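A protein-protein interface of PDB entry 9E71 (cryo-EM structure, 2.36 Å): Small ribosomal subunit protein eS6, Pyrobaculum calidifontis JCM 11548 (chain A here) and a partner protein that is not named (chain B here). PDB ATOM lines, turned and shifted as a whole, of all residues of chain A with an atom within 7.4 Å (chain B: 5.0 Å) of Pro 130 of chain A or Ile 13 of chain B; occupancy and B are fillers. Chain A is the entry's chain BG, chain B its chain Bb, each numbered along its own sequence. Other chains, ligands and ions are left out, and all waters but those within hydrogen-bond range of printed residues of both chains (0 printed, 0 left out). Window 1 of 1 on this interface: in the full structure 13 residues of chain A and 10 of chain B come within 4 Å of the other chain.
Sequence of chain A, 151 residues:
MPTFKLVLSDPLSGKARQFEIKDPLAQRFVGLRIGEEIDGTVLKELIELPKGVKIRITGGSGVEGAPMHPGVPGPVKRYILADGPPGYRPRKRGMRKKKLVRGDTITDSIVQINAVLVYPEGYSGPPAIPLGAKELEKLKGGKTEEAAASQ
Printed residues of chain B within 4 Å of Gly 125 of chain A: Thr 14 (3.5 Å).
Pro 130 of chain A touches four residues of chain B.
Of chain A, only Leu 12 (3.1 Å), Ser 13 (3.3 Å), Pro 127 (3.5 Å) and Pro 130 (3.9 Å) come within 4 Å of Ile 13 of chain B.
Printed residues of chain A within 4 Å of Thr 14 of chain B: Gly 125, Pro 126 and Pro 127.
The nearest residue of chain A that does not touch Ile 13 of chain B is Ile 129 of chain A (4.8 Å).
The nearest printed residue of chain A that does not touch Thr 14 of chain B is Leu 12 of chain A (6.6 Å).
O of Leu 12 of chain A lies within hydrogen-bond range of NH1 of Arg 17 of chain B (3.1 Å).
Of the 14 printed residues of chain B, 6 touch a printed residue of chain A.
Hydrophobic or aromatic side chains of chain B within 4 Å of the printed part of chain A: Ala 9, Ala 10 and Ile 13.
Hydrophobic or aromatic side chains of chain A within 4 Å of the printed part of chain B: Leu 12, Pro 126, Pro 127, Pro 130 and Leu 131.
The backbone NH (N) of Ser 13 of chain A is in hydrogen-bond range of the side-chain carboxylate (OD1) of Asp 10 of chain A (2.9 Å).
O of Lys 11 of chain B lies within hydrogen-bond range of OG1 of Thr 14 of chain B, 2.6 Å away.
The side-chain carboxylate (OD1) of Asp 10 of chain A lies within hydrogen-bond range of the backbone NH (N) of Leu 12 of chain A, 2.6 Å away.
The side-chain hydroxyl of Ser 13 of chain A lies within hydrogen-bond range of the backbone carbonyl oxygen of Ile 129 of chain A (2.6 Å).
The side-chain hydroxyl (OG) of Ser 13 of chain A lies close to the backbone NH (N) of Lys 15 of chain A, at 3.3 Å.
Leu 12 of chain A touches Ile 13 of chain B (O to CG2, 3.1 Å).
CD1 of Ile 13 of chain B touches CB of Ser 13 of chain A, 3.3 Å away.
Thr 14 of chain B touches Pro 126 of chain A.
Pro 127 of chain A touches Ala 10 of chain B (CD to O, 3.1 Å).
CD1 of Ile 13 of chain B touches CG of Pro 127 of chain A, 3.5 Å away.
Pro 127 of chain A touches Thr 14 of chain B (CD to CG2, 3.9 Å).
Glu 6 of chain B touches Pro 130 of chain A.
CB of Pro 130 of chain A touches CB of Ala 9 of chain B (3.8 Å).
CD1 of Ile 13 of chain B touches O of Pro 130 of chain A (3.9 Å).
Leu 131 of chain A touches Glu 6 of chain B.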
ATOM      1  N   ASP A  10       3.072   4.842  13.017  1.00  0.00           N
ATOM      2  CA  ASP A  10       3.814   6.016  13.448  1.00  0.00           C
ATOM      3  C   ASP A  10       4.844   5.471  14.429  1.00  0.00           C
ATOM      4  O   ASP A  10       4.457   4.930  15.477  1.00  0.00           O
ATOM      5  CB  ASP A  10       2.853   7.030  14.104  1.00  0.00           C
ATOM      6  CG  ASP A  10       3.516   8.135  14.997  1.00  0.00           C
ATOM      7  OD1 ASP A  10       4.728   8.215  15.303  1.00  0.00           O
ATOM      8  OD2 ASP A  10       2.721   8.983  15.452  1.00  0.00           O
ATOM      9  N   LEU A  12       6.693   7.059  16.446  1.00  0.00           N
ATOM     10  CA  LEU A  12       6.864   7.934  17.594  1.00  0.00           C
ATOM     11  C   LEU A  12       5.702   7.892  18.567  1.00  0.00           C
ATOM     12  O   LEU A  12       5.874   8.260  19.729  1.00  0.00           O
ATOM     13  CB  LEU A  12       7.075   9.381  17.136  1.00  0.00           C
ATOM     14  CG  LEU A  12       8.444   9.669  16.525  1.00  0.00           C
ATOM     15  CD1 LEU A  12       8.558  11.133  16.141  1.00  0.00           C
ATOM     16  CD2 LEU A  12       9.549   9.274  17.488  1.00  0.00           C
ATOM     17  N   SER A  13       4.527   7.460  18.120  1.00  0.00           N
ATOM     18  CA  SER A  13       3.370   7.299  18.985  1.00  0.00           C
ATOM     19  C   SER A  13       3.090   5.846  19.335  1.00  0.00           C
ATOM     20  O   SER A  13       2.326   5.585  20.269  1.00  0.00           O
ATOM     21  CB  SER A  13       2.131   7.909  18.325  1.00  0.00           C
ATOM     22  OG  SER A  13       1.027   7.026  18.396  1.00  0.00           O
ATOM     23  N   GLY A  14       3.680   4.901  18.608  1.00  0.00           N
ATOM     24  CA  GLY A  14       3.402   3.499  18.822  1.00  0.00           C
ATOM     25  C   GLY A  14       2.073   3.031  18.285  1.00  0.00           C
ATOM     26  O   GLY A  14       1.679   1.893  18.557  1.00  0.00           O
ATOM     27  N   LYS A  15       1.369   3.868  17.534  1.00  0.00           N
ATOM     28  CA  LYS A  15       0.055   3.544  17.004  1.00  0.00           C
ATOM     29  C   LYS A  15       0.129   3.326  15.499  1.00  0.00           C
ATOM     30  O   LYS A  15       1.143   3.596  14.845  1.00  0.00           O
ATOM     31  CB  LYS A  15      -0.956   4.648  17.331  1.00  0.00           C
ATOM     32  CG  LYS A  15      -1.592   4.536  18.706  1.00  0.00           C
ATOM     33  CD  LYS A  15      -0.608   4.896  19.801  1.00  0.00           C
ATOM     34  CE  LYS A  15      -1.292   5.005  21.150  1.00  0.00           C
ATOM     35  NZ  LYS A  15      -2.131   3.818  21.450  1.00  0.00           N
ATOM     36  N   TYR A 119      10.311   9.928  10.059  1.00  0.00           N
ATOM     37  CA  TYR A 119      10.377  11.337  10.386  1.00  0.00           C
ATOM     38  C   TYR A 119      11.735  11.903   9.978  1.00  0.00           C
ATOM     39  O   TYR A 119      12.723  11.169   9.904  1.00  0.00           O
ATOM     40  CB  TYR A 119      10.141  11.544  11.874  1.00  0.00           C
ATOM     41  CG  TYR A 119       8.713  11.288  12.282  1.00  0.00           C
ATOM     42  CD1 TYR A 119       7.725  12.224  12.030  1.00  0.00           C
ATOM     43  CD2 TYR A 119       8.350  10.103  12.904  1.00  0.00           C
ATOM     44  CE1 TYR A 119       6.416  11.996  12.398  1.00  0.00           C
ATOM     45  CE2 TYR A 119       7.041   9.864  13.275  1.00  0.00           C
ATOM     46  CZ  TYR A 119       6.079  10.816  13.019  1.00  0.00           C
ATOM     47  OH  TYR A 119       4.773  10.591  13.384  1.00  0.00           O
ATOM     48  N   GLY A 125       8.879  17.103  16.661  1.00  0.00           N
ATOM     49  CA  GLY A 125       7.527  17.610  16.679  1.00  0.00           C
ATOM     50  C   GLY A 125       6.527  16.637  17.269  1.00  0.00           C
ATOM     51  O   GLY A 125       6.878  15.719  18.017  1.00  0.00           O
ATOM     52  N   PRO A 126       5.250  16.834  16.954  1.00  0.00           N
ATOM     53  CA  PRO A 126       4.212  15.935  17.453  1.00  0.00           C
ATOM     54  C   PRO A 126       4.141  14.667  16.623  1.00  0.00           C
ATOM     55  O   PRO A 126       4.555  14.654  15.454  1.00  0.00           O
ATOM     56  CB  PRO A 126       2.933  16.769  17.304  1.00  0.00           C
ATOM     57  CG  PRO A 126       3.216  17.640  16.133  1.00  0.00           C
ATOM     58  CD  PRO A 126       4.685  17.966  16.200  1.00  0.00           C
ATOM     59  N   PRO A 127       3.621  13.579  17.191  1.00  0.00           N
ATOM     60  CA  PRO A 127       3.448  12.349  16.411  1.00  0.00           C
ATOM     61  C   PRO A 127       2.341  12.492  15.380  1.00  0.00           C
ATOM     62  O   PRO A 127       1.326  13.154  15.613  1.00  0.00           O
ATOM     63  CB  PRO A 127       3.083  11.309  17.475  1.00  0.00           C
ATOM     64  CG  PRO A 127       2.436  12.098  18.544  1.00  0.00           C
ATOM     65  CD  PRO A 127       3.141  13.426  18.573  1.00  0.00           C
ATOM     66  N   ALA A 128       2.543  11.841  14.231  1.00  0.00           N
ATOM     67  CA  ALA A 128       1.581  11.942  13.138  1.00  0.00           C
ATOM     68  C   ALA A 128       0.248  11.294  13.488  1.00  0.00           C
ATOM     69  O   ALA A 128      -0.798  11.726  12.991  1.00  0.00           O
ATOM     70  CB  ALA A 128       2.159  11.315  11.873  1.00  0.00           C
ATOM     71  N   ILE A 129       0.262  10.260  14.325  1.00  0.00           N
ATOM     72  CA  ILE A 129      -0.960   9.577  14.748  1.00  0.00           C
ATOM     73  C   ILE A 129      -0.987   9.514  16.271  1.00  0.00           C
ATOM     74  O   ILE A 129      -0.477   8.551  16.861  1.00  0.00           O
ATOM     75  CB  ILE A 129      -1.060   8.172  14.138  1.00  0.00           C
ATOM     76  CG1 ILE A 129      -1.124   8.253  12.614  1.00  0.00           C
ATOM     77  CG2 ILE A 129      -2.274   7.446  14.680  1.00  0.00           C
ATOM     78  CD1 ILE A 129      -1.066   6.910  11.930  1.00  0.00           C
ATOM     79  N   PRO A 130      -1.563  10.510  16.947  1.00  0.00           N
ATOM     80  CA  PRO A 130      -1.534  10.490  18.419  1.00  0.00           C
ATOM     81  C   PRO A 130      -2.396   9.401  19.029  1.00  0.00           C
ATOM     82  O   PRO A 130      -2.160   9.008  20.177  1.00  0.00           O
ATOM     83  CB  PRO A 130      -2.031  11.890  18.800  1.00  0.00           C
ATOM     84  CG  PRO A 130      -2.812  12.358  17.631  1.00  0.00           C
ATOM     85  CD  PRO A 130      -2.278  11.677  16.407  1.00  0.00           C
ATOM     86  N   LEU A 131      -3.392   8.904  18.302  1.00  0.00           N
ATOM     87  CA  LEU A 131      -4.260   7.851  18.809  1.00  0.00           C
ATOM     88  C   LEU A 131      -4.786   7.023  17.648  1.00  0.00           C
ATOM     89  O   LEU A 131      -4.863   7.496  16.512  1.00  0.00           O
ATOM     90  CB  LEU A 131      -5.434   8.421  19.614  1.00  0.00           C
ATOM     91  CG  LEU A 131      -5.082   8.936  21.008  1.00  0.00           C
ATOM     92  CD1 LEU A 131      -6.229   9.732  21.603  1.00  0.00           C
ATOM     93  CD2 LEU A 131      -4.697   7.778  21.914  1.00  0.00           C
ATOM     94  N   GLY A 132      -5.132   5.776  17.943  1.00  0.00           N
ATOM     95  CA  GLY A 132      -5.803   4.946  16.969  1.00  0.00           C
ATOM     96  C   GLY A 132      -7.281   5.269  16.889  1.00  0.00           C
ATOM     97  O   GLY A 132      -7.874   5.864  17.791  1.00  0.00           O
ATOM     98  N   GLU A 135      -9.178   3.046  19.337  1.00  0.00           N
ATOM     99  CA  GLU A 135      -8.808   3.510  20.669  1.00  0.00           C
ATOM    100  C   GLU A 135      -9.566   4.778  21.037  1.00  0.00           C
ATOM    101  O   GLU A 135     -10.100   4.897  22.145  1.00  0.00           O
ATOM    102  CB  GLU A 135      -7.302   3.752  20.737  1.00  0.00           C
ATOM    103  CG  GLU A 135      -6.736   3.746  22.140  1.00  0.00           C
ATOM    104  CD  GLU A 135      -5.230   3.850  22.146  1.00  0.00           C
ATOM    105  OE1 GLU A 135      -4.694   4.739  21.454  1.00  0.00           O
ATOM    106  OE2 GLU A 135      -4.578   3.041  22.838  1.00  0.00           O
ATOM    107  N   GLU B   6      -6.843  14.333  20.062  1.00  0.00           N
ATOM    108  CA  GLU B   6      -5.639  14.008  19.302  1.00  0.00           C
ATOM    109  C   GLU B   6      -4.531  15.025  19.540  1.00  0.00           C
ATOM    110  O   GLU B   6      -3.356  14.658  19.637  1.00  0.00           O
ATOM    111  CB  GLU B   6      -5.972  13.901  17.814  1.00  0.00           C
ATOM    112  CG  GLU B   6      -7.161  12.999  17.513  1.00  0.00           C
ATOM    113  CD  GLU B   6      -6.756  11.681  16.880  1.00  0.00           C
ATOM    114  OE1 GLU B   6      -5.542  11.441  16.719  1.00  0.00           O
ATOM    115  OE2 GLU B   6      -7.651  10.879  16.544  1.00  0.00           O
ATOM    116  N   ALA B   7      -4.887  16.309  19.643  1.00  0.00           N
ATOM    117  CA  ALA B   7      -3.891  17.333  19.948  1.00  0.00           C
ATOM    118  C   ALA B   7      -3.270  17.116  21.323  1.00  0.00           C
ATOM    119  O   ALA B   7      -2.040  17.175  21.472  1.00  0.00           O
ATOM    120  CB  ALA B   7      -4.524  18.719  19.859  1.00  0.00           C
ATOM    121  N   ALA B   9      -3.176  14.302  23.080  1.00  0.00           N
ATOM    122  CA  ALA B   9      -2.425  13.054  23.073  1.00  0.00           C
ATOM    123  C   ALA B   9      -1.083  13.224  22.384  1.00  0.00           C
ATOM    124  O   ALA B   9      -0.058  12.789  22.913  1.00  0.00           O
ATOM    125  CB  ALA B   9      -3.236  11.953  22.394  1.00  0.00           C
ATOM    126  N   ALA B  10      -1.066  13.889  21.221  1.00  0.00           N
ATOM    127  CA  ALA B  10       0.182  14.091  20.493  1.00  0.00           C
ATOM    128  C   ALA B  10       1.149  14.955  21.284  1.00  0.00           C
ATOM    129  O   ALA B  10       2.348  14.668  21.331  1.00  0.00           O
ATOM    130  CB  ALA B  10      -0.100  14.716  19.129  1.00  0.00           C
ATOM    131  N   LYS B  11       0.636  16.006  21.927  1.00  0.00           N
ATOM    132  CA  LYS B  11       1.461  16.855  22.780  1.00  0.00           C
ATOM    133  C   LYS B  11       2.042  16.043  23.938  1.00  0.00           C
ATOM    134  O   LYS B  11       3.217  16.208  24.303  1.00  0.00           O
ATOM    135  CB  LYS B  11       0.580  18.036  23.223  1.00  0.00           C
ATOM    136  CG  LYS B  11       1.112  19.217  24.078  1.00  0.00           C
ATOM    137  CD  LYS B  11       1.738  18.903  25.422  1.00  0.00           C
ATOM    138  CE  LYS B  11       0.826  18.010  26.254  1.00  0.00           C
ATOM    139  NZ  LYS B  11      -0.482  18.627  26.606  1.00  0.00           N
ATOM    140  N   LEU B  12       1.239  15.137  24.508  1.00  0.00           N
ATOM    141  CA  LEU B  12       1.740  14.263  25.564  1.00  0.00           C
ATOM    142  C   LEU B  12       2.853  13.354  25.059  1.00  0.00           C
ATOM    143  O   LEU B  12       3.844  13.136  25.766  1.00  0.00           O
ATOM    144  CB  LEU B  12       0.603  13.436  26.156  1.00  0.00           C
ATOM    145  CG  LEU B  12      -0.318  14.191  27.111  1.00  0.00           C
ATOM    146  CD1 LEU B  12      -1.335  13.245  27.727  1.00  0.00           C
ATOM    147  CD2 LEU B  12       0.501  14.885  28.192  1.00  0.00           C
ATOM    148  N   ILE B  13       2.716  12.824  23.839  1.00  0.00           N
ATOM    149  CA  ILE B  13       3.788  11.999  23.277  1.00  0.00           C
ATOM    150  C   ILE B  13       5.044  12.826  23.044  1.00  0.00           C
ATOM    151  O   ILE B  13       6.160  12.326  23.217  1.00  0.00           O
ATOM    152  CB  ILE B  13       3.354  11.279  21.986  1.00  0.00           C
ATOM    153  CG1 ILE B  13       1.919  10.789  22.070  1.00  0.00           C
ATOM    154  CG2 ILE B  13       4.264  10.103  21.706  1.00  0.00           C
ATOM    155  CD1 ILE B  13       1.544   9.803  21.004  1.00  0.00           C
ATOM    156  N   THR B  14       4.892  14.091  22.628  1.00  0.00           N
ATOM    157  CA  THR B  14       6.069  14.950  22.486  1.00  0.00           C
ATOM    158  C   THR B  14       6.781  15.138  23.814  1.00  0.00           C
ATOM    159  O   THR B  14       8.014  15.054  23.880  1.00  0.00           O
ATOM    160  CB  THR B  14       5.718  16.324  21.910  1.00  0.00           C
ATOM    161  OG1 THR B  14       5.179  17.161  22.941  1.00  0.00           O
ATOM    162  CG2 THR B  14       4.777  16.233  20.754  1.00  0.00           C
ATOM    163  N   ARG B  15       6.028  15.381  24.886  1.00  0.00           N
ATOM    164  CA  ARG B  15       6.697  15.559  26.169  1.00  0.00           C
ATOM    165  C   ARG B  15       7.309  14.245  26.644  1.00  0.00           C
ATOM    166  O   ARG B  15       8.369  14.239  27.275  1.00  0.00           O
ATOM    167  CB  ARG B  15       5.741  16.151  27.201  1.00  0.00           C
ATOM    168  CG  ARG B  15       4.854  17.228  26.596  1.00  0.00           C
ATOM    169  CD  ARG B  15       3.980  17.953  27.616  1.00  0.00           C
ATOM    170  NE  ARG B  15       4.600  18.234  28.904  1.00  0.00           N
ATOM    171  CZ  ARG B  15       5.771  18.837  29.079  1.00  0.00           C
ATOM    172  NH1 ARG B  15       6.408  19.444  28.088  1.00  0.00           N
ATOM    173  NH2 ARG B  15       6.282  18.909  30.293  1.00  0.00           N
ATOM    174  N   LEU B  16       6.693  13.113  26.289  1.00  0.00           N
ATOM    175  CA  LEU B  16       7.266  11.821  26.657  1.00  0.00           C
ATOM    176  C   LEU B  16       8.581  11.551  25.927  1.00  0.00           C
ATOM    177  O   LEU B  16       9.543  11.064  26.533  1.00  0.00           O
ATOM    178  CB  LEU B  16       6.260  10.701  26.389  1.00  0.00           C
ATOM    179  CG  LEU B  16       5.170  10.489  27.445  1.00  0.00           C
ATOM    180  CD1 LEU B  16       4.471   9.160  27.252  1.00  0.00           C
ATOM    181  CD2 LEU B  16       5.763  10.576  28.840  1.00  0.00           C
ATOM    182  N   ARG B  17       8.642  11.840  24.622  1.00  0.00           N
ATOM    183  CA  ARG B  17       9.893  11.630  23.892  1.00  0.00           C
ATOM    184  C   ARG B  17      10.961  12.622  24.327  1.00  0.00           C
ATOM    185  O   ARG B  17      12.151  12.288  24.354  1.00  0.00           O
ATOM    186  CB  ARG B  17       9.687  11.714  22.376  1.00  0.00           C
ATOM    187  CG  ARG B  17       8.445  11.044  21.830  1.00  0.00           C
ATOM    188  CD  ARG B  17       8.410   9.538  22.040  1.00  0.00           C
ATOM    189  NE  ARG B  17       9.226   8.832  21.059  1.00  0.00           N
ATOM    190  CZ  ARG B  17       9.082   7.552  20.748  1.00  0.00           C
ATOM    191  NH1 ARG B  17       8.128   6.813  21.286  1.00  0.00           N
ATOM    192  NH2 ARG B  17       9.896   7.005  19.850  1.00  0.00           N
ATOM    193  N   GLU B  18      10.573  13.849  24.677  1.00  0.00           N
ATOM    194  CA  GLU B  18      11.586  14.765  25.184  1.00  0.00           C
ATOM    195  C   GLU B  18      12.103  14.310  26.544  1.00  0.00           C
ATOM    196  O   GLU B  18      13.304  14.424  26.830  1.00  0.00           O
ATOM    197  CB  GLU B  18      11.061  16.199  25.243  1.00  0.00           C
ATOM    198  CG  GLU B  18      10.090  16.500  26.347  1.00  0.00           C
ATOM    199  CD  GLU B  18       9.292  17.748  26.069  1.00  0.00           C
ATOM    200  OE1 GLU B  18       9.529  18.760  26.757  1.00  0.00           O
ATOM    201  OE2 GLU B  18       8.458  17.735  25.143  1.00  0.00           O
ATOM    202  N   LEU B  51      -0.808   5.729  26.365  1.00  0.00           N
ATOM    203  CA  LEU B  51       0.610   6.043  26.462  1.00  0.00           C
ATOM    204  C   LEU B  51       1.374   5.017  27.285  1.00  0.00           C
ATOM    205  O   LEU B  51       2.446   5.334  27.810  1.00  0.00           O
ATOM    206  CB  LEU B  51       0.801   7.435  27.059  1.00  0.00           C
ATOM    207  CG  LEU B  51       0.012   8.580  26.428  1.00  0.00           C
ATOM    208  CD1 LEU B  51      -0.189   9.698  27.435  1.00  0.00           C
ATOM    209  CD2 LEU B  51       0.725   9.095  25.186  1.00  0.00           C
ATOM    210  N   LEU B  54       5.195   4.198  26.125  1.00  0.00           N
ATOM    211  CA  LEU B  54       6.181   5.241  26.382  1.00  0.00           C
ATOM    212  C   LEU B  54       6.382   5.468  27.873  1.00  0.00           C
ATOM    213  O   LEU B  54       7.491   5.804  28.304  1.00  0.00           O
ATOM    214  CB  LEU B  54       5.761   6.538  25.698  1.00  0.00           C
ATOM    215  CG  LEU B  54       6.352   6.793  24.312  1.00  0.00           C
ATOM    216  CD1 LEU B  54       7.842   7.070  24.409  1.00  0.00           C
ATOM    217  CD2 LEU B  54       6.084   5.617  23.387  1.00  0.00           C
